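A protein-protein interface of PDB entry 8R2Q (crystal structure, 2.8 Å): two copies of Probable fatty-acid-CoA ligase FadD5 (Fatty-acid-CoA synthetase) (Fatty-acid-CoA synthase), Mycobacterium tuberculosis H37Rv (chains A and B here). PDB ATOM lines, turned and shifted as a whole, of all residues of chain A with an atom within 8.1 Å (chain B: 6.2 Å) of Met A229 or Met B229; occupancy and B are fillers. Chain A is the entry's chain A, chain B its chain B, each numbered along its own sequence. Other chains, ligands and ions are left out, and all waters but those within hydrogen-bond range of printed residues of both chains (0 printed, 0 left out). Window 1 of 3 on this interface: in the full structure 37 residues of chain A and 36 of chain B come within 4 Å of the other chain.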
ATOM      1  N   GLN A  42      19.911  32.603  23.543  1.00  0.00           N
ATOM      2  CA  GLN A  42      19.854  33.025  22.149  1.00  0.00           C
ATOM      3  C   GLN A  42      18.393  33.183  21.748  1.00  0.00           C
ATOM      4  O   GLN A  42      17.668  32.192  21.618  1.00  0.00           O
ATOM      5  CB  GLN A  42      20.571  32.037  21.232  1.00  0.00           C
ATOM      6  CG  GLN A  42      21.974  32.471  20.814  1.00  0.00           C
ATOM      7  CD  GLN A  42      21.986  33.721  19.935  1.00  0.00           C
ATOM      8  OE1 GLN A  42      20.940  34.244  19.551  1.00  0.00           O
ATOM      9  NE2 GLN A  42      23.184  34.199  19.611  1.00  0.00           N
ATOM     10  N   GLN A  47      18.993  39.707  20.945  1.00  0.00           N
ATOM     11  CA  GLN A  47      19.739  40.280  19.831  1.00  0.00           C
ATOM     12  C   GLN A  47      19.321  41.721  19.579  1.00  0.00           C
ATOM     13  O   GLN A  47      20.160  42.569  19.251  1.00  0.00           O
ATOM     14  CB  GLN A  47      19.540  39.429  18.579  1.00  0.00           C
ATOM     15  CG  GLN A  47      19.932  37.980  18.767  1.00  0.00           C
ATOM     16  CD  GLN A  47      19.189  37.052  17.832  1.00  0.00           C
ATOM     17  OE1 GLN A  47      18.513  37.497  16.905  1.00  0.00           O
ATOM     18  NE2 GLN A  47      19.300  35.753  18.077  1.00  0.00           N
ATOM     19  N   ALA A 222      14.903  28.170  20.189  1.00  0.00           N
ATOM     20  CA  ALA A 222      15.912  27.283  19.621  1.00  0.00           C
ATOM     21  C   ALA A 222      15.534  26.862  18.208  1.00  0.00           C
ATOM     22  O   ALA A 222      16.398  26.752  17.330  1.00  0.00           O
ATOM     23  CB  ALA A 222      16.102  26.058  20.515  1.00  0.00           C
ATOM     24  N   ASN A 223      14.242  26.624  17.974  1.00  0.00           N
ATOM     25  CA  ASN A 223      13.758  26.327  16.632  1.00  0.00           C
ATOM     26  C   ASN A 223      14.137  27.438  15.661  1.00  0.00           C
ATOM     27  O   ASN A 223      14.762  27.195  14.623  1.00  0.00           O
ATOM     28  CB  ASN A 223      12.241  26.129  16.668  1.00  0.00           C
ATOM     29  CG  ASN A 223      11.683  25.615  15.358  1.00  0.00           C
ATOM     30  OD1 ASN A 223      11.571  26.354  14.380  1.00  0.00           O
ATOM     31  ND2 ASN A 223      11.307  24.345  15.339  1.00  0.00           N
ATOM     32  N   LEU A 224      13.776  28.679  15.998  1.00  0.00           N
ATOM     33  CA  LEU A 224      14.049  29.803  15.111  1.00  0.00           C
ATOM     34  C   LEU A 224      15.546  30.026  14.937  1.00  0.00           C
ATOM     35  O   LEU A 224      16.004  30.389  13.846  1.00  0.00           O
ATOM     36  CB  LEU A 224      13.372  31.062  15.652  1.00  0.00           C
ATOM     37  CG  LEU A 224      11.861  30.944  15.859  1.00  0.00           C
ATOM     38  CD1 LEU A 224      11.307  32.189  16.525  1.00  0.00           C
ATOM     39  CD2 LEU A 224      11.167  30.694  14.534  1.00  0.00           C
ATOM     40  N   THR A 225      16.329  29.817  16.000  1.00  0.00           N
ATOM     41  CA  THR A 225      17.777  29.955  15.889  1.00  0.00           C
ATOM     42  C   THR A 225      18.339  28.970  14.873  1.00  0.00           C
ATOM     43  O   THR A 225      19.156  29.336  14.019  1.00  0.00           O
ATOM     44  CB  THR A 225      18.440  29.749  17.252  1.00  0.00           C
ATOM     45  OG1 THR A 225      17.832  30.610  18.221  1.00  0.00           O
ATOM     46  CG2 THR A 225      19.926  30.068  17.168  1.00  0.00           C
ATOM     47  N   GLY A 226      17.906  27.712  14.946  1.00  0.00           N
ATOM     48  CA  GLY A 226      18.385  26.723  13.997  1.00  0.00           C
ATOM     49  C   GLY A 226      17.951  27.018  12.574  1.00  0.00           C
ATOM     50  O   GLY A 226      18.713  26.807  11.627  1.00  0.00           O
ATOM     51  N   GLN A 227      16.722  27.511  12.401  1.00  0.00           N
ATOM     52  CA  GLN A 227      16.267  27.882  11.066  1.00  0.00           C
ATOM     53  C   GLN A 227      17.081  29.038  10.503  1.00  0.00           C
ATOM     54  O   GLN A 227      17.345  29.080   9.294  1.00  0.00           O
ATOM     55  CB  GLN A 227      14.781  28.240  11.091  1.00  0.00           C
ATOM     56  CG  GLN A 227      13.876  27.107  11.546  1.00  0.00           C
ATOM     57  CD  GLN A 227      12.575  27.052  10.770  1.00  0.00           C
ATOM     58  OE1 GLN A 227      12.565  27.196   9.546  1.00  0.00           O
ATOM     59  NE2 GLN A 227      11.470  26.841  11.478  1.00  0.00           N
ATOM     60  N   ALA A 228      17.488  29.980  11.357  1.00  0.00           N
ATOM     61  CA  ALA A 228      18.372  31.049  10.906  1.00  0.00           C
ATOM     62  C   ALA A 228      19.725  30.501  10.482  1.00  0.00           C
ATOM     63  O   ALA A 228      20.357  31.047   9.569  1.00  0.00           O
ATOM     64  CB  ALA A 228      18.541  32.096  12.009  1.00  0.00           C
ATOM     65  N   MET A 229      20.180  29.425  11.127  1.00  0.00           N
ATOM     66  CA  MET A 229      21.454  28.825  10.748  1.00  0.00           C
ATOM     67  C   MET A 229      21.392  28.269   9.332  1.00  0.00           C
ATOM     68  O   MET A 229      22.343  28.422   8.555  1.00  0.00           O
ATOM     69  CB  MET A 229      21.831  27.734  11.749  1.00  0.00           C
ATOM     70  CG  MET A 229      23.305  27.372  11.762  1.00  0.00           C
ATOM     71  SD  MET A 229      23.743  26.382  13.203  1.00  0.00           S
ATOM     72  CE  MET A 229      22.669  24.960  12.994  1.00  0.00           C
ATOM     73  N   THR A 230      20.273  27.634   8.973  1.00  0.00           N
ATOM     74  CA  THR A 230      20.114  27.108   7.620  1.00  0.00           C
ATOM     75  C   THR A 230      20.248  28.214   6.582  1.00  0.00           C
ATOM     76  O   THR A 230      20.882  28.023   5.538  1.00  0.00           O
ATOM     77  CB  THR A 230      18.762  26.405   7.483  1.00  0.00           C
ATOM     78  OG1 THR A 230      18.705  25.288   8.378  1.00  0.00           O
ATOM     79  CG2 THR A 230      18.559  25.913   6.059  1.00  0.00           C
ATOM     80  N   ALA A 231      19.667  29.385   6.860  1.00  0.00           N
ATOM     81  CA  ALA A 231      19.819  30.514   5.950  1.00  0.00           C
ATOM     82  C   ALA A 231      21.274  30.938   5.824  1.00  0.00           C
ATOM     83  O   ALA A 231      21.691  31.419   4.764  1.00  0.00           O
ATOM     84  CB  ALA A 231      18.965  31.693   6.421  1.00  0.00           C
ATOM     85  N   LEU A 232      22.066  30.751   6.882  1.00  0.00           N
ATOM     86  CA  LEU A 232      23.443  31.228   6.861  1.00  0.00           C
ATOM     87  C   LEU A 232      24.320  30.384   5.942  1.00  0.00           C
ATOM     88  O   LEU A 232      25.167  30.926   5.225  1.00  0.00           O
ATOM     89  CB  LEU A 232      24.011  31.254   8.280  1.00  0.00           C
ATOM     90  CG  LEU A 232      23.427  32.337   9.187  1.00  0.00           C
ATOM     91  CD1 LEU A 232      24.078  32.305  10.563  1.00  0.00           C
ATOM     92  CD2 LEU A 232      23.590  33.702   8.540  1.00  0.00           C
ATOM     93  N   TYR A 233      24.143  29.062   5.943  1.00  0.00           N
ATOM     94  CA  TYR A 233      24.998  28.209   5.127  1.00  0.00           C
ATOM     95  C   TYR A 233      24.397  27.879   3.769  1.00  0.00           C
ATOM     96  O   TYR A 233      24.990  27.099   3.017  1.00  0.00           O
ATOM     97  CB  TYR A 233      25.372  26.919   5.878  1.00  0.00           C
ATOM     98  CG  TYR A 233      24.250  25.977   6.276  1.00  0.00           C
ATOM     99  CD1 TYR A 233      23.615  25.173   5.335  1.00  0.00           C
ATOM    100  CD2 TYR A 233      23.877  25.839   7.608  1.00  0.00           C
ATOM    101  CE1 TYR A 233      22.612  24.294   5.705  1.00  0.00           C
ATOM    102  CE2 TYR A 233      22.878  24.961   7.988  1.00  0.00           C
ATOM    103  CZ  TYR A 233      22.248  24.191   7.032  1.00  0.00           C
ATOM    104  OH  TYR A 233      21.253  23.318   7.411  1.00  0.00           O
ATOM    105  N   THR A 234      23.250  28.460   3.427  1.00  0.00           N
ATOM    106  CA  THR A 234      22.720  28.376   2.073  1.00  0.00           C
ATOM    107  C   THR A 234      22.848  29.707   1.345  1.00  0.00           C
ATOM    108  O   THR A 234      23.482  29.777   0.287  1.00  0.00           O
ATOM    109  CB  THR A 234      21.256  27.913   2.089  1.00  0.00           C
ATOM    110  OG1 THR A 234      20.472  28.812   2.884  1.00  0.00           O
ATOM    111  CG2 THR A 234      21.150  26.515   2.664  1.00  0.00           C
ATOM    112  N   SER A 235      22.271  30.776   1.896  1.00  0.00           N
ATOM    113  CA  SER A 235      22.335  32.091   1.273  1.00  0.00           C
ATOM    114  C   SER A 235      23.611  32.847   1.611  1.00  0.00           C
ATOM    115  O   SER A 235      23.910  33.849   0.952  1.00  0.00           O
ATOM    116  CB  SER A 235      21.125  32.935   1.691  1.00  0.00           C
ATOM    117  OG  SER A 235      19.907  32.264   1.429  1.00  0.00           O
ATOM    118  N   GLY A 236      24.365  32.403   2.608  1.00  0.00           N
ATOM    119  CA  GLY A 236      25.515  33.157   3.060  1.00  0.00           C
ATOM    120  C   GLY A 236      25.087  34.458   3.716  1.00  0.00           C
ATOM    121  O   GLY A 236      23.904  34.746   3.903  1.00  0.00           O
ATOM    122  N   ALA A 237      26.086  35.262   4.068  1.00  0.00           N
ATOM    123  CA  ALA A 237      25.822  36.544   4.703  1.00  0.00           C
ATOM    124  C   ALA A 237      27.043  37.438   4.572  1.00  0.00           C
ATOM    125  O   ALA A 237      28.178  36.970   4.685  1.00  0.00           O
ATOM    126  CB  ALA A 237      25.455  36.370   6.179  1.00  0.00           C
ATOM    127  N   LEU A 260      14.643  36.410  10.330  1.00  0.00           N
ATOM    128  CA  LEU A 260      15.608  35.784  11.230  1.00  0.00           C
ATOM    129  C   LEU A 260      17.019  36.301  10.986  1.00  0.00           C
ATOM    130  O   LEU A 260      17.754  36.593  11.937  1.00  0.00           O
ATOM    131  CB  LEU A 260      15.568  34.264  11.069  1.00  0.00           C
ATOM    132  CG  LEU A 260      14.251  33.556  11.377  1.00  0.00           C
ATOM    133  CD1 LEU A 260      14.393  32.062  11.155  1.00  0.00           C
ATOM    134  CD2 LEU A 260      13.809  33.848  12.798  1.00  0.00           C
ATOM    135  N   THR A 261      17.414  36.423   9.718  1.00  0.00           N
ATOM    136  CA  THR A 261      18.777  36.833   9.397  1.00  0.00           C
ATOM    137  C   THR A 261      19.039  38.273   9.823  1.00  0.00           C
ATOM    138  O   THR A 261      20.072  38.570  10.435  1.00  0.00           O
ATOM    139  CB  THR A 261      19.036  36.647   7.901  1.00  0.00           C
ATOM    140  OG1 THR A 261      19.483  35.305   7.662  1.00  0.00           O
ATOM    141  CG2 THR A 261      20.086  37.629   7.396  1.00  0.00           C
ATOM    142  N   LEU A 264      19.172  38.545  13.653  1.00  0.00           N
ATOM    143  CA  LEU A 264      20.331  37.862  14.218  1.00  0.00           C
ATOM    144  C   LEU A 264      21.620  38.623  13.926  1.00  0.00           C
ATOM    145  O   LEU A 264      22.432  38.858  14.829  1.00  0.00           O
ATOM    146  CB  LEU A 264      20.419  36.438  13.672  1.00  0.00           C
ATOM    147  CG  LEU A 264      21.694  35.669  14.021  1.00  0.00           C
ATOM    148  CD1 LEU A 264      21.759  35.380  15.513  1.00  0.00           C
ATOM    149  CD2 LEU A 264      21.790  34.383  13.213  1.00  0.00           C
ATOM    150  N   LEU A 265      21.824  39.013  12.671  1.00  0.00           N
ATOM    151  CA  LEU A 265      23.069  39.631  12.233  1.00  0.00           C
ATOM    152  C   LEU A 265      23.068  41.147  12.361  1.00  0.00           C
ATOM    153  O   LEU A 265      24.087  41.775  12.058  1.00  0.00           O
ATOM    154  CB  LEU A 265      23.361  39.246  10.782  1.00  0.00           C
ATOM    155  CG  LEU A 265      23.367  37.747  10.488  1.00  0.00           C
ATOM    156  CD1 LEU A 265      23.514  37.499   8.998  1.00  0.00           C
ATOM    157  CD2 LEU A 265      24.476  37.058  11.263  1.00  0.00           C
ATOM    158  N   ILE A 376      19.174  19.034   3.590  1.00  0.00           N
ATOM    159  CA  ILE A 376      20.184  19.924   4.161  1.00  0.00           C
ATOM    160  C   ILE A 376      20.948  19.201   5.267  1.00  0.00           C
ATOM    161  O   ILE A 376      20.425  18.245   5.860  1.00  0.00           O
ATOM    162  CB  ILE A 376      19.542  21.224   4.672  1.00  0.00           C
ATOM    163  CG1 ILE A 376      18.552  20.935   5.797  1.00  0.00           C
ATOM    164  CG2 ILE A 376      18.854  21.953   3.531  1.00  0.00           C
ATOM    165  CD1 ILE A 376      18.115  22.174   6.533  1.00  0.00           C
ATOM    166  N   PRO A 377      22.180  19.619   5.580  1.00  0.00           N
ATOM    167  CA  PRO A 377      23.019  18.823   6.493  1.00  0.00           C
ATOM    168  C   PRO A 377      22.513  18.750   7.924  1.00  0.00           C
ATOM    169  O   PRO A 377      22.928  17.840   8.653  1.00  0.00           O
ATOM    170  CB  PRO A 377      24.378  19.533   6.428  1.00  0.00           C
ATOM    171  CG  PRO A 377      24.356  20.289   5.141  1.00  0.00           C
ATOM    172  CD  PRO A 377      22.937  20.724   4.967  1.00  0.00           C
ATOM    173  N   THR A 378      21.654  19.671   8.362  1.00  0.00           N
ATOM    174  CA  THR A 378      21.158  19.676   9.732  1.00  0.00           C
ATOM    175  C   THR A 378      19.780  19.036   9.850  1.00  0.00           C
ATOM    176  O   THR A 378      19.017  19.367  10.763  1.00  0.00           O
ATOM    177  CB  THR A 378      21.133  21.100  10.289  1.00  0.00           C
ATOM    178  OG1 THR A 378      20.229  21.903   9.520  1.00  0.00           O
ATOM    179  CG2 THR A 378      22.525  21.713  10.234  1.00  0.00           C
ATOM    180  N   PRO A 404      16.418  19.166  15.093  1.00  0.00           N
ATOM    181  CA  PRO A 404      16.106  20.054  16.223  1.00  0.00           C
ATOM    182  C   PRO A 404      15.175  21.184  15.834  1.00  0.00           C
ATOM    183  O   PRO A 404      14.426  21.680  16.684  1.00  0.00           O
ATOM    184  CB  PRO A 404      17.483  20.585  16.655  1.00  0.00           C
ATOM    185  CG  PRO A 404      18.491  19.705  15.967  1.00  0.00           C
ATOM    186  CD  PRO A 404      17.836  19.241  14.708  1.00  0.00           C
ATOM    187  N   THR A 405      15.195  21.600  14.570  1.00  0.00           N
ATOM    188  CA  THR A 405      14.389  22.707  14.079  1.00  0.00           C
ATOM    189  C   THR A 405      12.966  22.298  13.715  1.00  0.00           C
ATOM    190  O   THR A 405      12.299  23.029  12.970  1.00  0.00           O
ATOM    191  CB  THR A 405      15.073  23.351  12.872  1.00  0.00           C
ATOM    192  OG1 THR A 405      15.373  22.345  11.896  1.00  0.00           O
ATOM    193  CG2 THR A 405      16.361  24.006  13.297  1.00  0.00           C
ATOM    194  N   GLN B  42      21.690  19.271  19.606  1.00  0.00           N
ATOM    195  CA  GLN B  42      22.562  19.787  18.552  1.00  0.00           C
ATOM    196  C   GLN B  42      24.004  19.731  19.046  1.00  0.00           C
ATOM    197  O   GLN B  42      24.419  20.558  19.864  1.00  0.00           O
ATOM    198  CB  GLN B  42      22.173  21.205  18.151  1.00  0.00           C
ATOM    199  CG  GLN B  42      23.059  21.809  17.065  1.00  0.00           C
ATOM    200  CD  GLN B  42      23.021  21.025  15.764  1.00  0.00           C
ATOM    201  OE1 GLN B  42      23.717  20.021  15.608  1.00  0.00           O
ATOM    202  NE2 GLN B  42      22.206  21.484  14.820  1.00  0.00           N
ATOM    203  N   LEU B 224      30.200  25.581  21.168  1.00  0.00           N
ATOM    204  CA  LEU B 224      30.788  25.197  19.887  1.00  0.00           C
ATOM    205  C   LEU B 224      29.822  25.436  18.732  1.00  0.00           C
ATOM    206  O   LEU B 224      30.236  25.850  17.643  1.00  0.00           O
ATOM    207  CB  LEU B 224      31.221  23.733  19.932  1.00  0.00           C
ATOM    208  CG  LEU B 224      32.356  23.425  20.908  1.00  0.00           C
ATOM    209  CD1 LEU B 224      32.646  21.937  20.930  1.00  0.00           C
ATOM    210  CD2 LEU B 224      33.601  24.215  20.534  1.00  0.00           C
ATOM    211  N   THR B 225      28.530  25.175  18.947  1.00  0.00           N
ATOM    212  CA  THR B 225      27.548  25.436  17.900  1.00  0.00           C
ATOM    213  C   THR B 225      27.508  26.918  17.550  1.00  0.00           C
ATOM    214  O   THR B 225      27.533  27.292  16.373  1.00  0.00           O
ATOM    215  CB  THR B 225      26.165  24.950  18.340  1.00  0.00           C
ATOM    216  OG1 THR B 225      26.252  23.589  18.775  1.00  0.00           O
ATOM    217  CG2 THR B 225      25.178  25.045  17.184  1.00  0.00           C
ATOM    218  N   GLY B 226      27.456  27.780  18.570  1.00  0.00           N
ATOM    219  CA  GLY B 226      27.436  29.211  18.321  1.00  0.00           C
ATOM    220  C   GLY B 226      28.699  29.716  17.649  1.00  0.00           C
ATOM    221  O   GLY B 226      28.655  30.688  16.891  1.00  0.00           O
ATOM    222  N   GLN B 227      29.838  29.074  17.918  1.00  0.00           N
ATOM    223  CA  GLN B 227      31.070  29.460  17.240  1.00  0.00           C
ATOM    224  C   GLN B 227      31.054  29.021  15.782  1.00  0.00           C
ATOM    225  O   GLN B 227      31.581  29.724  14.912  1.00  0.00           O
ATOM    226  CB  GLN B 227      32.282  28.875  17.962  1.00  0.00           C
ATOM    227  CG  GLN B 227      32.487  29.419  19.363  1.00  0.00           C
ATOM    228  CD  GLN B 227      33.950  29.481  19.747  1.00  0.00           C
ATOM    229  OE1 GLN B 227      34.774  30.025  19.010  1.00  0.00           O
ATOM    230  NE2 GLN B 227      34.281  28.920  20.903  1.00  0.00           N
ATOM    231  N   ALA B 228      30.464  27.856  15.498  1.00  0.00           N
ATOM    232  CA  ALA B 228      30.268  27.450  14.112  1.00  0.00           C
ATOM    233  C   ALA B 228      29.349  28.418  13.381  1.00  0.00           C
ATOM    234  O   ALA B 228      29.534  28.672  12.185  1.00  0.00           O
ATOM    235  CB  ALA B 228      29.701  26.032  14.049  1.00  0.00           C
ATOM    236  N   MET B 229      28.361  28.971  14.084  1.00  0.00           N
ATOM    237  CA  MET B 229      27.475  29.953  13.470  1.00  0.00           C
ATOM    238  C   MET B 229      28.243  31.202  13.056  1.00  0.00           C
ATOM    239  O   MET B 229      27.977  31.780  11.996  1.00  0.00           O
ATOM    240  CB  MET B 229      26.346  30.300  14.440  1.00  0.00           C
ATOM    241  CG  MET B 229      25.286  31.209  13.864  1.00  0.00           C
ATOM    242  SD  MET B 229      23.835  31.282  14.927  1.00  0.00           S
ATOM    243  CE  MET B 229      23.340  29.560  14.923  1.00  0.00           C
ATOM    244  N   THR B 230      29.207  31.627  13.877  1.00  0.00           N
ATOM    245  CA  THR B 230      30.035  32.774  13.517  1.00  0.00           C
ATOM    246  C   THR B 230      30.846  32.490  12.261  1.00  0.00           C
ATOM    247  O   THR B 230      30.999  33.363  11.399  1.00  0.00           O
ATOM    248  CB  THR B 230      30.955  33.148  14.679  1.00  0.00           C
ATOM    249  OG1 THR B 230      30.165  33.501  15.821  1.00  0.00           O
ATOM    250  CG2 THR B 230      31.842  34.324  14.298  1.00  0.00           C
ATOM    251  N   ALA B 231      31.370  31.269  12.137  1.00  0.00           N
ATOM    252  CA  ALA B 231      32.058  30.887  10.910  1.00  0.00           C
ATOM    253  C   ALA B 231      31.127  30.943   9.709  1.00  0.00           C
ATOM    254  O   ALA B 231      31.573  31.217   8.590  1.00  0.00           O
ATOM    255  CB  ALA B 231      32.649  29.484  11.053  1.00  0.00           C
ATOM    256  N   LEU B 232      29.830  30.710   9.926  1.00  0.00           N
ATOM    257  CA  LEU B 232      28.893  30.582   8.817  1.00  0.00           C
ATOM    258  C   LEU B 232      28.529  31.928   8.207  1.00  0.00           C
ATOM    259  O   LEU B 232      28.425  32.040   6.981  1.00  0.00           O
ATOM    260  CB  LEU B 232      27.632  29.850   9.275  1.00  0.00           C
ATOM    261  CG  LEU B 232      27.771  28.338   9.454  1.00  0.00           C
ATOM    262  CD1 LEU B 232      26.433  27.721   9.818  1.00  0.00           C
ATOM    263  CD2 LEU B 232      28.328  27.705   8.190  1.00  0.00           C
ATOM    264  N   TYR B 233      28.321  32.959   9.026  1.00  0.00           N
ATOM    265  CA  TYR B 233      27.939  34.260   8.489  1.00  0.00           C
ATOM    266  C   TYR B 233      29.137  35.158   8.193  1.00  0.00           C
ATOM    267  O   TYR B 233      28.947  36.322   7.827  1.00  0.00           O
ATOM    268  CB  TYR B 233      26.944  34.969   9.419  1.00  0.00           C
ATOM    269  CG  TYR B 233      27.409  35.303  10.823  1.00  0.00           C
ATOM    270  CD1 TYR B 233      28.282  36.357  11.061  1.00  0.00           C
ATOM    271  CD2 TYR B 233      26.910  34.610  11.918  1.00  0.00           C
ATOM    272  CE1 TYR B 233      28.679  36.679  12.347  1.00  0.00           C
ATOM    273  CE2 TYR B 233      27.300  34.926  13.205  1.00  0.00           C
ATOM    274  CZ  TYR B 233      28.185  35.961  13.415  1.00  0.00           C
ATOM    275  OH  TYR B 233      28.578  36.278  14.696  1.00  0.00           O
ATOM    276  N   THR B 234      30.356  34.643   8.327  1.00  0.00           N
ATOM    277  CA  THR B 234      31.552  35.348   7.892  1.00  0.00           C
ATOM    278  C   THR B 234      32.195  34.665   6.691  1.00  0.00           C
ATOM    279  O   THR B 234      32.272  35.255   5.609  1.00  0.00           O
ATOM    280  CB  THR B 234      32.555  35.458   9.048  1.00  0.00           C
ATOM    281  OG1 THR B 234      32.776  34.162   9.617  1.00  0.00           O
ATOM    282  CG2 THR B 234      32.027  36.399  10.119  1.00  0.00           C
ATOM    283  N   LEU B 264      29.558  20.020  11.045  1.00  0.00           N
ATOM    284  CA  LEU B 264      28.169  20.460  11.000  1.00  0.00           C
ATOM    285  C   LEU B 264      27.567  20.223   9.623  1.00  0.00           C
ATOM    286  O   LEU B 264      26.536  19.554   9.489  1.00  0.00           O
ATOM    287  CB  LEU B 264      28.078  21.939  11.382  1.00  0.00           C
ATOM    288  CG  LEU B 264      26.703  22.598  11.284  1.00  0.00           C
ATOM    289  CD1 LEU B 264      25.749  22.012  12.310  1.00  0.00           C
ATOM    290  CD2 LEU B 264      26.820  24.106  11.453  1.00  0.00           C
ATOM    291  N   THR B 378      26.837  38.590  17.070  1.00  0.00           N
ATOM    292  CA  THR B 378      26.402  37.691  18.132  1.00  0.00           C
ATOM    293  C   THR B 378      27.206  37.878  19.413  1.00  0.00           C
ATOM    294  O   THR B 378      27.216  36.987  20.268  1.00  0.00           O
ATOM    295  CB  THR B 378      26.477  36.239  17.664  1.00  0.00           C
ATOM    296  OG1 THR B 378      27.810  35.939  17.233  1.00  0.00           O
ATOM    297  CG2 THR B 378      25.509  36.005  16.515  1.00  0.00           C
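The backbone carbonyl oxygen (O) of Ala A237 sits close to the backbone carbonyl oxygen (O) of Tyr B233 (3.3 Å).
Of the 14 printed residues of chain B, 6 touch a printed residue of chain A.
Hydrophobic or aromatic side chains of chain B within 4 Å of the printed part of chain A: Met B229, Leu B232, Tyr B233 and Leu B264.
Of the 27 printed residues of chain A, 8 touch a printed residue of chain B.
Hydrophobic or aromatic side chains of chain A within 4 Å of the printed part of chain B: Met A229, Leu A232, Tyr A233, Ala A237, Leu A264, Leu A265 and Pro A377.
Along chain A the printed residues that touch a printed residue of chain B span positions 229 to 378.
Among the printed residues, 12 pairs touch across the chains.
Gly A226 touches none of the printed residues of chain B.
Of chain B, only Gln B42 (3.95 Å), Met B229 (3.6 Å) and Leu B232 (3.7 Å) come within 4 Å of Met A229.
Printed residues of chain B within 4 Å of Ala A237: Tyr B233.
Of the printed residues of chain B, Leu A264 touches Thr B378.
Ile A376 touches none of the printed residues of chain B.
Of the printed residues of chain B, Pro A377 touches Leu B264 (3.7 Å).
Printed residues of chain B within 4 Å of Thr A378: Leu B264.
Met B229 touches just these residues of chain A: Met A229 (3.6 Å) and Leu A232 (3.7 Å).
The nearest residue of chain B that does not touch Met A229 is Leu B264 (4.2 Å).
Met A229 touches Met B229.
Met A229 touches Leu B232 (CG to CD1, 3.7 Å).
Leu A232 touches Met B229 (CD1 to CG, 3.7 Å).
O of Leu B232 touches O of Leu A232 (3.9 Å).
Leu A232 touches Tyr B233 (CD2 to CB, 3.7 Å).
Tyr A233 touches Leu B232.
Leu A264 touches Thr B378 (CD1 to CG2, 3.9 Å).
Tyr B233 touches Leu A265 (CG to CD2, 3.4 Å).
Pro A377 touches Leu B264 (CB to O, 3.7 Å).
CD1 of Leu B264 touches CG2 of Thr A378, at 3.8 Å.
Met A229 touches Gln B42, but with the chains exchanged Gln A42 does not touch Met B229 (5.6 Å).
Met A229 touches its own counterpart, Met B229.
Met A229 touches Leu B232, and with the chains exchanged Leu A232 touches Met B229.
Leu A264 touches Thr B378, and with the chains exchanged Thr A378 touches Leu B264.
Positions printed for both chains: 42, 224, 225, 226, 227, 228, 229, 230, 231, 232, 233, 234, 264 and 378.
The side-chain amide oxygen (OE1) of Gln A47 sits close to the backbone NH (N) of Leu A264 (3.5 Å).
The side-chain hydroxyl of Tyr A233 lies within hydrogen-bond range of the side-chain hydroxyl of Thr A230 (3.4 Å).
The side-chain hydroxyl (OH) of Tyr A233 is in hydrogen-bond range of the side-chain hydroxyl (OG1) of Thr A378 (2.7 Å).
OG1 of Thr B230 is in hydrogen-bond range of OH of Tyr B233 (3.4 Å).
OH of Tyr B233 is in hydrogen-bond range of OG1 of Thr B378 (2.7 Å).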
